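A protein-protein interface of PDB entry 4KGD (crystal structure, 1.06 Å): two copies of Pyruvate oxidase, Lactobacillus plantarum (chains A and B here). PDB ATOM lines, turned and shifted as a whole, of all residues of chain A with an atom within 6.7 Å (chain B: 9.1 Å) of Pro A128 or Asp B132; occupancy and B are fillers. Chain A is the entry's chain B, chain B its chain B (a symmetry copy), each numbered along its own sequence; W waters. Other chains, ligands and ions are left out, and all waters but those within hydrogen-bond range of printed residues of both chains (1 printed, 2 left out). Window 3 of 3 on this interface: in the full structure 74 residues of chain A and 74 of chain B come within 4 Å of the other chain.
Of the 20 printed residues of chain B, 5 touch a printed residue of chain A.
Hydrophobic or aromatic side chains of chain B that line the printed part of chain A: Tyr B95, Pro B128, Ile B129 and Phe B419.
Of the 11 printed residues of chain A, 4 touch a printed residue of chain B.
Among the printed residues, 6 pairs touch across the chains.
Pro A128 touches Asp B132, and with the chains exchanged Asp A132 touches Pro B128.
Ile A129 touches Asp B132, and with the chains exchanged Asp A132 touches Ile B129.
Of the 6 pairs that touch across the chains among the printed residues, 4 have their exchanged pair printed and touching as well.
Among the printed residues, pairs that only touch across the chains: Met A124 with Phe B419 (3.8 Å), Pro A128 with Asp B132 (3.4 Å), Ile A129 with Tyr B95 (3.5 Å), Ile A129 with Asp B132 (3.6 Å), Asp A132 with Pro B128 (3.4 Å) and Asp A132 with Ile B129 (3.6 Å).
Water W1 lies within hydrogen-bond range of the side-chain carboxylate (OD2) of Asp B132, the backbone carbonyl oxygen (O) of Asn A125 and the guanidinium group (NH2) of Arg B98.
The side-chain hydroxyl (OH) of Tyr B95 lies within hydrogen-bond range of the side-chain carboxylate (OD2) of Asp B132, 2.7 Å away.
The guanidinium group (NH1) of Arg B98 lies within salt-bridge range of the side-chain carboxylate (OD2) of Asp B132 (3.0 Å).
Of the printed residues of chain B, Pro A128 touches Asp B132.
Asp B132 touches just these residues of chain A: Pro A128 and Ile A129.
Ile A129 touches just these residues of chain B: Tyr B95 (3.5 Å) and Asp B132 (3.6 Å).
Of the printed residues of chain A, Pro B128 touches Asp A132.
Of the printed residues of chain A, Tyr B95 touches Ile A129 (3.5 Å).
Of the printed residues of chain B, Met A124 touches Phe B419.
The nearest printed residue of chain B that does not touch Asp A132 is Glu B126 (6.2 Å).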
ATOM      1  N   MET A 124     -11.581 -26.808 -11.808  1.00  0.00           N
ATOM      2  CA  MET A 124     -12.808 -26.334 -11.154  1.00  0.00           C
ATOM      3  C   MET A 124     -13.742 -25.906 -12.266  1.00  0.00           C
ATOM      4  O   MET A 124     -13.341 -25.669 -13.389  1.00  0.00           O
ATOM      5  CB  MET A 124     -12.437 -25.238 -10.174  1.00  0.00           C
ATOM      6  CG  MET A 124     -12.044 -23.959 -10.821  1.00  0.00           C
ATOM      7  SD  MET A 124     -10.962 -22.974  -9.769  1.00  0.00           S
ATOM      8  CE  MET A 124      -9.504 -24.038  -9.936  1.00  0.00           C
ATOM      9  N   ASN A 125     -15.009 -25.724 -11.887  1.00  0.00           N
ATOM     10  CA  ASN A 125     -15.963 -25.058 -12.784  1.00  0.00           C
ATOM     11  C   ASN A 125     -15.636 -23.587 -12.770  1.00  0.00           C
ATOM     12  O   ASN A 125     -15.886 -22.900 -11.773  1.00  0.00           O
ATOM     13  CB  ASN A 125     -17.384 -25.373 -12.307  1.00  0.00           C
ATOM     14  CG  ASN A 125     -18.397 -24.594 -13.126  1.00  0.00           C
ATOM     15  OD1 ASN A 125     -18.080 -24.045 -14.210  1.00  0.00           O
ATOM     16  ND2 ASN A 125     -19.593 -24.538 -12.584  1.00  0.00           N
ATOM     17  N   GLU A 126     -15.036 -23.075 -13.833  1.00  0.00           N
ATOM     18  CA  GLU A 126     -14.588 -21.700 -13.866  1.00  0.00           C
ATOM     19  C   GLU A 126     -15.648 -20.732 -14.303  1.00  0.00           C
ATOM     20  O   GLU A 126     -15.474 -19.519 -14.089  1.00  0.00           O
ATOM     21  CB  GLU A 126     -13.340 -21.579 -14.717  1.00  0.00           C
ATOM     22  CG  GLU A 126     -12.109 -22.253 -14.093  1.00  0.00           C
ATOM     23  CD  GLU A 126     -10.886 -21.997 -14.938  1.00  0.00           C
ATOM     24  OE1 GLU A 126     -10.861 -22.601 -16.078  1.00  0.00           O
ATOM     25  OE2 GLU A 126     -10.003 -21.260 -14.546  1.00  0.00           O
ATOM     26  N   ASN A 127     -16.729 -21.204 -14.903  1.00  0.00           N
ATOM     27  CA  ASN A 127     -17.709 -20.264 -15.427  1.00  0.00           C
ATOM     28  C   ASN A 127     -18.299 -19.352 -14.352  1.00  0.00           C
ATOM     29  O   ASN A 127     -18.471 -18.146 -14.606  1.00  0.00           O
ATOM     30  CB  ASN A 127     -18.749 -21.039 -16.236  1.00  0.00           C
ATOM     31  CG  ASN A 127     -19.667 -20.114 -17.002  1.00  0.00           C
ATOM     32  OD1 ASN A 127     -20.805 -19.860 -16.596  1.00  0.00           O
ATOM     33  ND2 ASN A 127     -19.178 -19.595 -18.107  1.00  0.00           N
ATOM     34  N   PRO A 128     -18.670 -19.844 -13.161  1.00  0.00           N
ATOM     35  CA  PRO A 128     -19.256 -18.923 -12.181  1.00  0.00           C
ATOM     36  C   PRO A 128     -18.331 -17.833 -11.698  1.00  0.00           C
ATOM     37  O   PRO A 128     -18.803 -16.828 -11.177  1.00  0.00           O
ATOM     38  CB  PRO A 128     -19.628 -19.845 -10.977  1.00  0.00           C
ATOM     39  CG  PRO A 128     -19.621 -21.225 -11.527  1.00  0.00           C
ATOM     40  CD  PRO A 128     -18.743 -21.256 -12.703  1.00  0.00           C
ATOM     41  N   ILE A 129     -17.033 -18.016 -11.841  1.00  0.00           N
ATOM     42  CA  ILE A 129     -16.070 -17.037 -11.357  1.00  0.00           C
ATOM     43  C   ILE A 129     -16.292 -15.693 -12.040  1.00  0.00           C
ATOM     44  O   ILE A 129     -16.109 -14.643 -11.435  1.00  0.00           O
ATOM     45  CB  ILE A 129     -14.640 -17.553 -11.550  1.00  0.00           C
ATOM     46  CG1 ILE A 129     -14.408 -18.902 -10.829  1.00  0.00           C
ATOM     47  CG2 ILE A 129     -13.628 -16.502 -11.133  1.00  0.00           C
ATOM     48  CD1 ILE A 129     -13.043 -19.478 -11.096  1.00  0.00           C
ATOM     49  N   TYR A 130     -16.605 -15.743 -13.352  1.00  0.00           N
ATOM     50  CA  TYR A 130     -16.646 -14.565 -14.216  1.00  0.00           C
ATOM     51  C   TYR A 130     -18.030 -14.079 -14.536  1.00  0.00           C
ATOM     52  O   TYR A 130     -18.164 -13.113 -15.282  1.00  0.00           O
ATOM     53  CB  TYR A 130     -15.856 -14.856 -15.541  1.00  0.00           C
ATOM     54  CG  TYR A 130     -14.444 -15.285 -15.195  1.00  0.00           C
ATOM     55  CD1 TYR A 130     -13.469 -14.357 -14.909  1.00  0.00           C
ATOM     56  CD2 TYR A 130     -14.077 -16.602 -15.047  1.00  0.00           C
ATOM     57  CE1 TYR A 130     -12.176 -14.713 -14.557  1.00  0.00           C
ATOM     58  CE2 TYR A 130     -12.806 -16.999 -14.638  1.00  0.00           C
ATOM     59  CZ  TYR A 130     -11.856 -16.048 -14.381  1.00  0.00           C
ATOM     60  OH  TYR A 130     -10.594 -16.354 -13.936  1.00  0.00           O
ATOM     61  N   ALA A 131     -19.052 -14.698 -13.950  1.00  0.00           N
ATOM     62  CA  ALA A 131     -20.426 -14.377 -14.330  1.00  0.00           C
ATOM     63  C   ALA A 131     -20.784 -12.925 -13.996  1.00  0.00           C
ATOM     64  O   ALA A 131     -21.521 -12.287 -14.716  1.00  0.00           O
ATOM     65  CB  ALA A 131     -21.383 -15.366 -13.668  1.00  0.00           C
ATOM     66  N   ASP A 132     -20.290 -12.401 -12.869  1.00  0.00           N
ATOM     67  CA  ASP A 132     -20.668 -11.049 -12.501  1.00  0.00           C
ATOM     68  C   ASP A 132     -19.940  -9.998 -13.326  1.00  0.00           C
ATOM     69  O   ASP A 132     -20.534  -8.978 -13.706  1.00  0.00           O
ATOM     70  CB  ASP A 132     -20.388 -10.854 -10.997  1.00  0.00           C
ATOM     71  CG  ASP A 132     -20.734  -9.420 -10.619  1.00  0.00           C
ATOM     72  OD1 ASP A 132     -21.921  -9.053 -10.607  1.00  0.00           O
ATOM     73  OD2 ASP A 132     -19.788  -8.652 -10.266  1.00  0.00           O
ATOM     74  N   ASN A 137     -19.748 -14.678 -21.142  1.00  0.00           N
ATOM     75  CA  ASN A 137     -18.993 -15.531 -20.244  1.00  0.00           C
ATOM     76  C   ASN A 137     -19.276 -17.005 -20.528  1.00  0.00           C
ATOM     77  O   ASN A 137     -20.286 -17.530 -20.048  1.00  0.00           O
ATOM     78  CB  ASN A 137     -19.401 -15.201 -18.792  1.00  0.00           C
ATOM     79  CG  ASN A 137     -18.742 -16.148 -17.799  1.00  0.00           C
ATOM     80  OD1 ASN A 137     -17.580 -16.479 -17.936  1.00  0.00           O
ATOM     81  ND2 ASN A 137     -19.533 -16.547 -16.794  1.00  0.00           N
ATOM     82  N   GLN A 167     -13.552 -19.310 -21.264  1.00  0.00           N
ATOM     83  CA  GLN A 167     -12.762 -20.360 -20.654  1.00  0.00           C
ATOM     84  C   GLN A 167     -12.494 -21.425 -21.703  1.00  0.00           C
ATOM     85  O   GLN A 167     -13.426 -21.906 -22.350  1.00  0.00           O
ATOM     86  CB  GLN A 167     -13.449 -20.974 -19.440  1.00  0.00           C
ATOM     87  CG  GLN A 167     -13.829 -19.979 -18.361  1.00  0.00           C
ATOM     88  CD  GLN A 167     -15.195 -19.381 -18.406  1.00  0.00           C
ATOM     89  OE1 GLN A 167     -16.198 -20.057 -18.681  1.00  0.00           O
ATOM     90  NE2 GLN A 167     -15.286 -18.079 -18.120  1.00  0.00           N
ATOM     91  N   MET B  91      -9.235 -12.465  -3.902  1.00  0.00           N
ATOM     92  CA  MET B  91      -9.685 -13.715  -4.510  1.00  0.00           C
ATOM     93  C   MET B  91      -8.687 -14.859  -4.490  1.00  0.00           C
ATOM     94  O   MET B  91      -9.077 -15.984  -4.201  1.00  0.00           O
ATOM     95  CB  MET B  91     -10.140 -13.437  -5.953  1.00  0.00           C
ATOM     96  CG  MET B  91     -11.488 -12.797  -6.031  1.00  0.00           C
ATOM     97  SD  MET B  91     -12.762 -13.781  -5.241  1.00  0.00           S
ATOM     98  CE  MET B  91     -14.136 -12.732  -5.530  1.00  0.00           C
ATOM     99  N   LEU B  94      -8.824 -16.389  -1.168  1.00  0.00           N
ATOM    100  CA  LEU B  94     -10.103 -17.006  -0.839  1.00  0.00           C
ATOM    101  C   LEU B  94     -10.300 -18.325  -1.589  1.00  0.00           C
ATOM    102  O   LEU B  94     -10.773 -19.290  -1.025  1.00  0.00           O
ATOM    103  CB  LEU B  94     -11.260 -16.053  -1.123  1.00  0.00           C
ATOM    104  CG  LEU B  94     -11.197 -14.708  -0.369  1.00  0.00           C
ATOM    105  CD1 LEU B  94     -12.433 -13.882  -0.657  1.00  0.00           C
ATOM    106  CD2 LEU B  94     -10.975 -14.873   1.117  1.00  0.00           C
ATOM    107  N   TYR B  95      -9.909 -18.366  -2.878  1.00  0.00           N
ATOM    108  CA  TYR B  95      -9.995 -19.619  -3.616  1.00  0.00           C
ATOM    109  C   TYR B  95      -9.023 -20.654  -3.057  1.00  0.00           C
ATOM    110  O   TYR B  95      -9.336 -21.844  -3.011  1.00  0.00           O
ATOM    111  CB  TYR B  95      -9.760 -19.395  -5.145  1.00  0.00           C
ATOM    112  CG  TYR B  95     -11.040 -18.995  -5.808  1.00  0.00           C
ATOM    113  CD1 TYR B  95     -11.927 -19.940  -6.300  1.00  0.00           C
ATOM    114  CD2 TYR B  95     -11.445 -17.652  -5.933  1.00  0.00           C
ATOM    115  CE1 TYR B  95     -13.128 -19.611  -6.890  1.00  0.00           C
ATOM    116  CE2 TYR B  95     -12.666 -17.324  -6.472  1.00  0.00           C
ATOM    117  CZ  TYR B  95     -13.509 -18.286  -6.964  1.00  0.00           C
ATOM    118  OH  TYR B  95     -14.734 -17.922  -7.451  1.00  0.00           O
ATOM    119  N   ARG B  98     -10.869 -22.076  -0.109  1.00  0.00           N
ATOM    120  CA  ARG B  98     -11.932 -22.963  -0.528  1.00  0.00           C
ATOM    121  C   ARG B  98     -11.350 -24.297  -0.951  1.00  0.00           C
ATOM    122  O   ARG B  98     -11.796 -25.372  -0.481  1.00  0.00           O
ATOM    123  CB  ARG B  98     -12.721 -22.378  -1.698  1.00  0.00           C
ATOM    124  CG  ARG B  98     -13.891 -23.294  -2.076  1.00  0.00           C
ATOM    125  CD  ARG B  98     -14.695 -22.857  -3.272  1.00  0.00           C
ATOM    126  NE  ARG B  98     -13.993 -23.156  -4.511  1.00  0.00           N
ATOM    127  CZ  ARG B  98     -14.440 -22.845  -5.709  1.00  0.00           C
ATOM    128  NH1 ARG B  98     -15.534 -22.126  -5.843  1.00  0.00           N
ATOM    129  NH2 ARG B  98     -13.765 -23.185  -6.783  1.00  0.00           N
ATOM    130  N   GLU B  99     -10.359 -24.288  -1.805  1.00  0.00           N
ATOM    131  CA  GLU B  99      -9.828 -25.524  -2.380  1.00  0.00           C
ATOM    132  C   GLU B  99      -9.028 -26.342  -1.394  1.00  0.00           C
ATOM    133  O   GLU B  99      -9.036 -27.592  -1.457  1.00  0.00           O
ATOM    134  CB  GLU B  99      -8.999 -25.196  -3.630  1.00  0.00           C
ATOM    135  CG  GLU B  99      -9.883 -24.645  -4.756  1.00  0.00           C
ATOM    136  CD  GLU B  99     -10.952 -25.564  -5.256  1.00  0.00           C
ATOM    137  OE1 GLU B  99     -10.717 -26.788  -5.450  1.00  0.00           O
ATOM    138  OE2 GLU B  99     -12.114 -25.130  -5.377  1.00  0.00           O
ATOM    139  N   GLU B 126     -22.004  -6.034  -4.576  1.00  0.00           N
ATOM    140  CA  GLU B 126     -20.845  -6.866  -4.334  1.00  0.00           C
ATOM    141  C   GLU B 126     -21.180  -8.306  -4.078  1.00  0.00           C
ATOM    142  O   GLU B 126     -20.272  -9.153  -4.151  1.00  0.00           O
ATOM    143  CB  GLU B 126     -20.010  -6.282  -3.213  1.00  0.00           C
ATOM    144  CG  GLU B 126     -19.325  -4.960  -3.588  1.00  0.00           C
ATOM    145  CD  GLU B 126     -18.426  -4.498  -2.468  1.00  0.00           C
ATOM    146  OE1 GLU B 126     -19.030  -4.089  -1.403  1.00  0.00           O
ATOM    147  OE2 GLU B 126     -17.217  -4.527  -2.588  1.00  0.00           O
ATOM    148  N   ASN B 127     -22.430  -8.623  -3.781  1.00  0.00           N
ATOM    149  CA  ASN B 127     -22.740  -9.999  -3.424  1.00  0.00           C
ATOM    150  C   ASN B 127     -22.401 -10.997  -4.532  1.00  0.00           C
ATOM    151  O   ASN B 127     -21.870 -12.081  -4.231  1.00  0.00           O
ATOM    152  CB  ASN B 127     -24.187 -10.066  -2.937  1.00  0.00           C
ATOM    153  CG  ASN B 127     -24.515 -11.413  -2.333  1.00  0.00           C
ATOM    154  OD1 ASN B 127     -25.144 -12.264  -2.969  1.00  0.00           O
ATOM    155  ND2 ASN B 127     -24.083 -11.620  -1.109  1.00  0.00           N
ATOM    156  N   PRO B 128     -22.707 -10.734  -5.811  1.00  0.00           N
ATOM    157  CA  PRO B 128     -22.381 -11.742  -6.824  1.00  0.00           C
ATOM    158  C   PRO B 128     -20.908 -12.021  -6.997  1.00  0.00           C
ATOM    159  O   PRO B 128     -20.550 -13.064  -7.531  1.00  0.00           O
ATOM    160  CB  PRO B 128     -22.942 -11.136  -8.149  1.00  0.00           C
ATOM    161  CG  PRO B 128     -23.889 -10.074  -7.721  1.00  0.00           C
ATOM    162  CD  PRO B 128     -23.503  -9.615  -6.382  1.00  0.00           C
ATOM    163  N   ILE B 129     -20.054 -11.109  -6.573  1.00  0.00           N
ATOM    164  CA  ILE B 129     -18.617 -11.277  -6.747  1.00  0.00           C
ATOM    165  C   ILE B 129     -18.141 -12.535  -6.030  1.00  0.00           C
ATOM    166  O   ILE B 129     -17.234 -13.215  -6.494  1.00  0.00           O
ATOM    167  CB  ILE B 129     -17.872 -10.025  -6.271  1.00  0.00           C
ATOM    168  CG1 ILE B 129     -18.336  -8.755  -7.022  1.00  0.00           C
ATOM    169  CG2 ILE B 129     -16.371 -10.226  -6.362  1.00  0.00           C
ATOM    170  CD1 ILE B 129     -17.694  -7.498  -6.495  1.00  0.00           C
ATOM    171  N   TYR B 130     -18.712 -12.784  -4.833  1.00  0.00           N
ATOM    172  CA  TYR B 130     -18.237 -13.815  -3.913  1.00  0.00           C
ATOM    173  C   TYR B 130     -19.082 -15.055  -3.882  1.00  0.00           C
ATOM    174  O   TYR B 130     -18.778 -15.964  -3.114  1.00  0.00           O
ATOM    175  CB  TYR B 130     -18.109 -13.213  -2.468  1.00  0.00           C
ATOM    176  CG  TYR B 130     -17.201 -11.999  -2.514  1.00  0.00           C
ATOM    177  CD1 TYR B 130     -15.833 -12.134  -2.495  1.00  0.00           C
ATOM    178  CD2 TYR B 130     -17.673 -10.717  -2.675  1.00  0.00           C
ATOM    179  CE1 TYR B 130     -14.971 -11.049  -2.568  1.00  0.00           C
ATOM    180  CE2 TYR B 130     -16.842  -9.609  -2.812  1.00  0.00           C
ATOM    181  CZ  TYR B 130     -15.484  -9.780  -2.769  1.00  0.00           C
ATOM    182  OH  TYR B 130     -14.596  -8.745  -2.935  1.00  0.00           O
ATOM    183  N   ALA B 131     -20.103 -15.127  -4.733  1.00  0.00           N
ATOM    184  CA  ALA B 131     -21.053 -16.235  -4.655  1.00  0.00           C
ATOM    185  C   ALA B 131     -20.382 -17.581  -4.948  1.00  0.00           C
ATOM    186  O   ALA B 131     -20.732 -18.587  -4.369  1.00  0.00           O
ATOM    187  CB  ALA B 131     -22.228 -15.967  -5.594  1.00  0.00           C
ATOM    188  N   ASP B 132     -19.431 -17.616  -5.887  1.00  0.00           N
ATOM    189  CA  ASP B 132     -18.828 -18.892  -6.226  1.00  0.00           C
ATOM    190  C   ASP B 132     -17.829 -19.359  -5.177  1.00  0.00           C
ATOM    191  O   ASP B 132     -17.763 -20.557  -4.866  1.00  0.00           O
ATOM    192  CB  ASP B 132     -18.152 -18.763  -7.606  1.00  0.00           C
ATOM    193  CG  ASP B 132     -17.473 -20.085  -7.942  1.00  0.00           C
ATOM    194  OD1 ASP B 132     -18.161 -21.086  -8.197  1.00  0.00           O
ATOM    195  OD2 ASP B 132     -16.206 -20.104  -8.007  1.00  0.00           O
ATOM    196  N   VAL B 133     -17.015 -18.450  -4.629  1.00  0.00           N
ATOM    197  CA  VAL B 133     -15.943 -18.863  -3.736  1.00  0.00           C
ATOM    198  C   VAL B 133     -16.453 -19.269  -2.355  1.00  0.00           C
ATOM    199  O   VAL B 133     -15.817 -20.066  -1.666  1.00  0.00           O
ATOM    200  CB  VAL B 133     -14.845 -17.789  -3.609  1.00  0.00           C
ATOM    201  CG1 VAL B 133     -15.278 -16.585  -2.784  1.00  0.00           C
ATOM    202  CG2 VAL B 133     -13.550 -18.414  -3.100  1.00  0.00           C
ATOM    203  N   ALA B 134     -17.563 -18.681  -1.931  1.00  0.00           N
ATOM    204  CA  ALA B 134     -17.965 -18.663  -0.538  1.00  0.00           C
ATOM    205  C   ALA B 134     -18.980 -19.734  -0.166  1.00  0.00           C
ATOM    206  O   ALA B 134     -19.945 -19.975  -0.868  1.00  0.00           O
ATOM    207  CB  ALA B 134     -18.556 -17.310  -0.217  1.00  0.00           C
ATOM    208  N   ASP B 135     -18.761 -20.357   0.992  1.00  0.00           N
ATOM    209  CA  ASP B 135     -19.772 -21.175   1.622  1.00  0.00           C
ATOM    210  C   ASP B 135     -20.964 -20.356   2.123  1.00  0.00           C
ATOM    211  O   ASP B 135     -22.089 -20.868   2.138  1.00  0.00           O
ATOM    212  CB  ASP B 135     -19.112 -21.952   2.779  1.00  0.00           C
ATOM    213  CG  ASP B 135     -20.076 -22.834   3.490  1.00  0.00           C
ATOM    214  OD1 ASP B 135     -20.348 -23.921   2.984  1.00  0.00           O
ATOM    215  OD2 ASP B 135     -20.593 -22.386   4.565  1.00  0.00           O
ATOM    216  N   TYR B 136     -20.686 -19.151   2.582  1.00  0.00           N
ATOM    217  CA  TYR B 136     -21.673 -18.231   3.159  1.00  0.00           C
ATOM    218  C   TYR B 136     -21.314 -16.864   2.617  1.00  0.00           C
ATOM    219  O   TYR B 136     -20.138 -16.509   2.623  1.00  0.00           O
ATOM    220  CB  TYR B 136     -21.607 -18.245   4.653  1.00  0.00           C
ATOM    221  CG  TYR B 136     -22.633 -17.414   5.376  1.00  0.00           C
ATOM    222  CD1 TYR B 136     -23.980 -17.734   5.329  1.00  0.00           C
ATOM    223  CD2 TYR B 136     -22.231 -16.310   6.169  1.00  0.00           C
ATOM    224  CE1 TYR B 136     -24.940 -17.005   6.005  1.00  0.00           C
ATOM    225  CE2 TYR B 136     -23.177 -15.576   6.877  1.00  0.00           C
ATOM    226  CZ  TYR B 136     -24.498 -15.917   6.791  1.00  0.00           C
ATOM    227  OH  TYR B 136     -25.411 -15.163   7.499  1.00  0.00           O
ATOM    228  N   ASN B 137     -22.275 -16.118   2.087  1.00  0.00           N
ATOM    229  CA  ASN B 137     -21.999 -14.916   1.322  1.00  0.00           C
ATOM    230  C   ASN B 137     -23.164 -13.932   1.418  1.00  0.00           C
ATOM    231  O   ASN B 137     -24.143 -14.080   0.681  1.00  0.00           O
ATOM    232  CB  ASN B 137     -21.782 -15.311  -0.154  1.00  0.00           C
ATOM    233  CG  ASN B 137     -21.615 -14.084  -1.040  1.00  0.00           C
ATOM    234  OD1 ASN B 137     -20.952 -13.136  -0.666  1.00  0.00           O
ATOM    235  ND2 ASN B 137     -22.230 -14.161  -2.228  1.00  0.00           N
ATOM    236  N   VAL B 163     -14.925 -20.744   3.161  1.00  0.00           N
ATOM    237  CA  VAL B 163     -14.879 -19.308   3.227  1.00  0.00           C
ATOM    238  C   VAL B 163     -16.258 -18.715   3.502  1.00  0.00           C
ATOM    239  O   VAL B 163     -17.227 -19.045   2.844  1.00  0.00           O
ATOM    240  CB  VAL B 163     -14.327 -18.726   1.892  1.00  0.00           C
ATOM    241  CG1 VAL B 163     -14.324 -17.207   1.922  1.00  0.00           C
ATOM    242  CG2 VAL B 163     -12.940 -19.262   1.599  1.00  0.00           C
ATOM    243  N   VAL B 165     -18.014 -14.906   3.635  1.00  0.00           N
ATOM    244  CA  VAL B 165     -17.831 -13.531   3.217  1.00  0.00           C
ATOM    245  C   VAL B 165     -19.022 -12.692   3.652  1.00  0.00           C
ATOM    246  O   VAL B 165     -20.169 -13.063   3.404  1.00  0.00           O
ATOM    247  CB  VAL B 165     -17.657 -13.421   1.662  1.00  0.00           C
ATOM    248  CG1 VAL B 165     -17.365 -11.987   1.287  1.00  0.00           C
ATOM    249  CG2 VAL B 165     -16.547 -14.333   1.190  1.00  0.00           C
ATOM    250  N   PHE B 419      -5.585 -25.318  -5.420  1.00  0.00           N
ATOM    251  CA  PHE B 419      -5.697 -24.143  -6.259  1.00  0.00           C
ATOM    252  C   PHE B 419      -4.357 -23.783  -6.857  1.00  0.00           C
ATOM    253  O   PHE B 419      -4.282 -23.204  -7.939  1.00  0.00           O
ATOM    254  CB  PHE B 419      -6.313 -22.980  -5.447  1.00  0.00           C
ATOM    255  CG  PHE B 419      -6.756 -21.786  -6.270  1.00  0.00           C
ATOM    256  CD1 PHE B 419      -7.734 -21.931  -7.255  1.00  0.00           C
ATOM    257  CD2 PHE B 419      -6.230 -20.512  -6.009  1.00  0.00           C
ATOM    258  CE1 PHE B 419      -8.184 -20.808  -7.965  1.00  0.00           C
ATOM    259  CE2 PHE B 419      -6.688 -19.408  -6.744  1.00  0.00           C
ATOM    260  CZ  PHE B 419      -7.640 -19.557  -7.718  1.00  0.00           C
HETATM  261  O   HOH W   1     -14.949 -22.251  -9.204  1.00  0.00           O
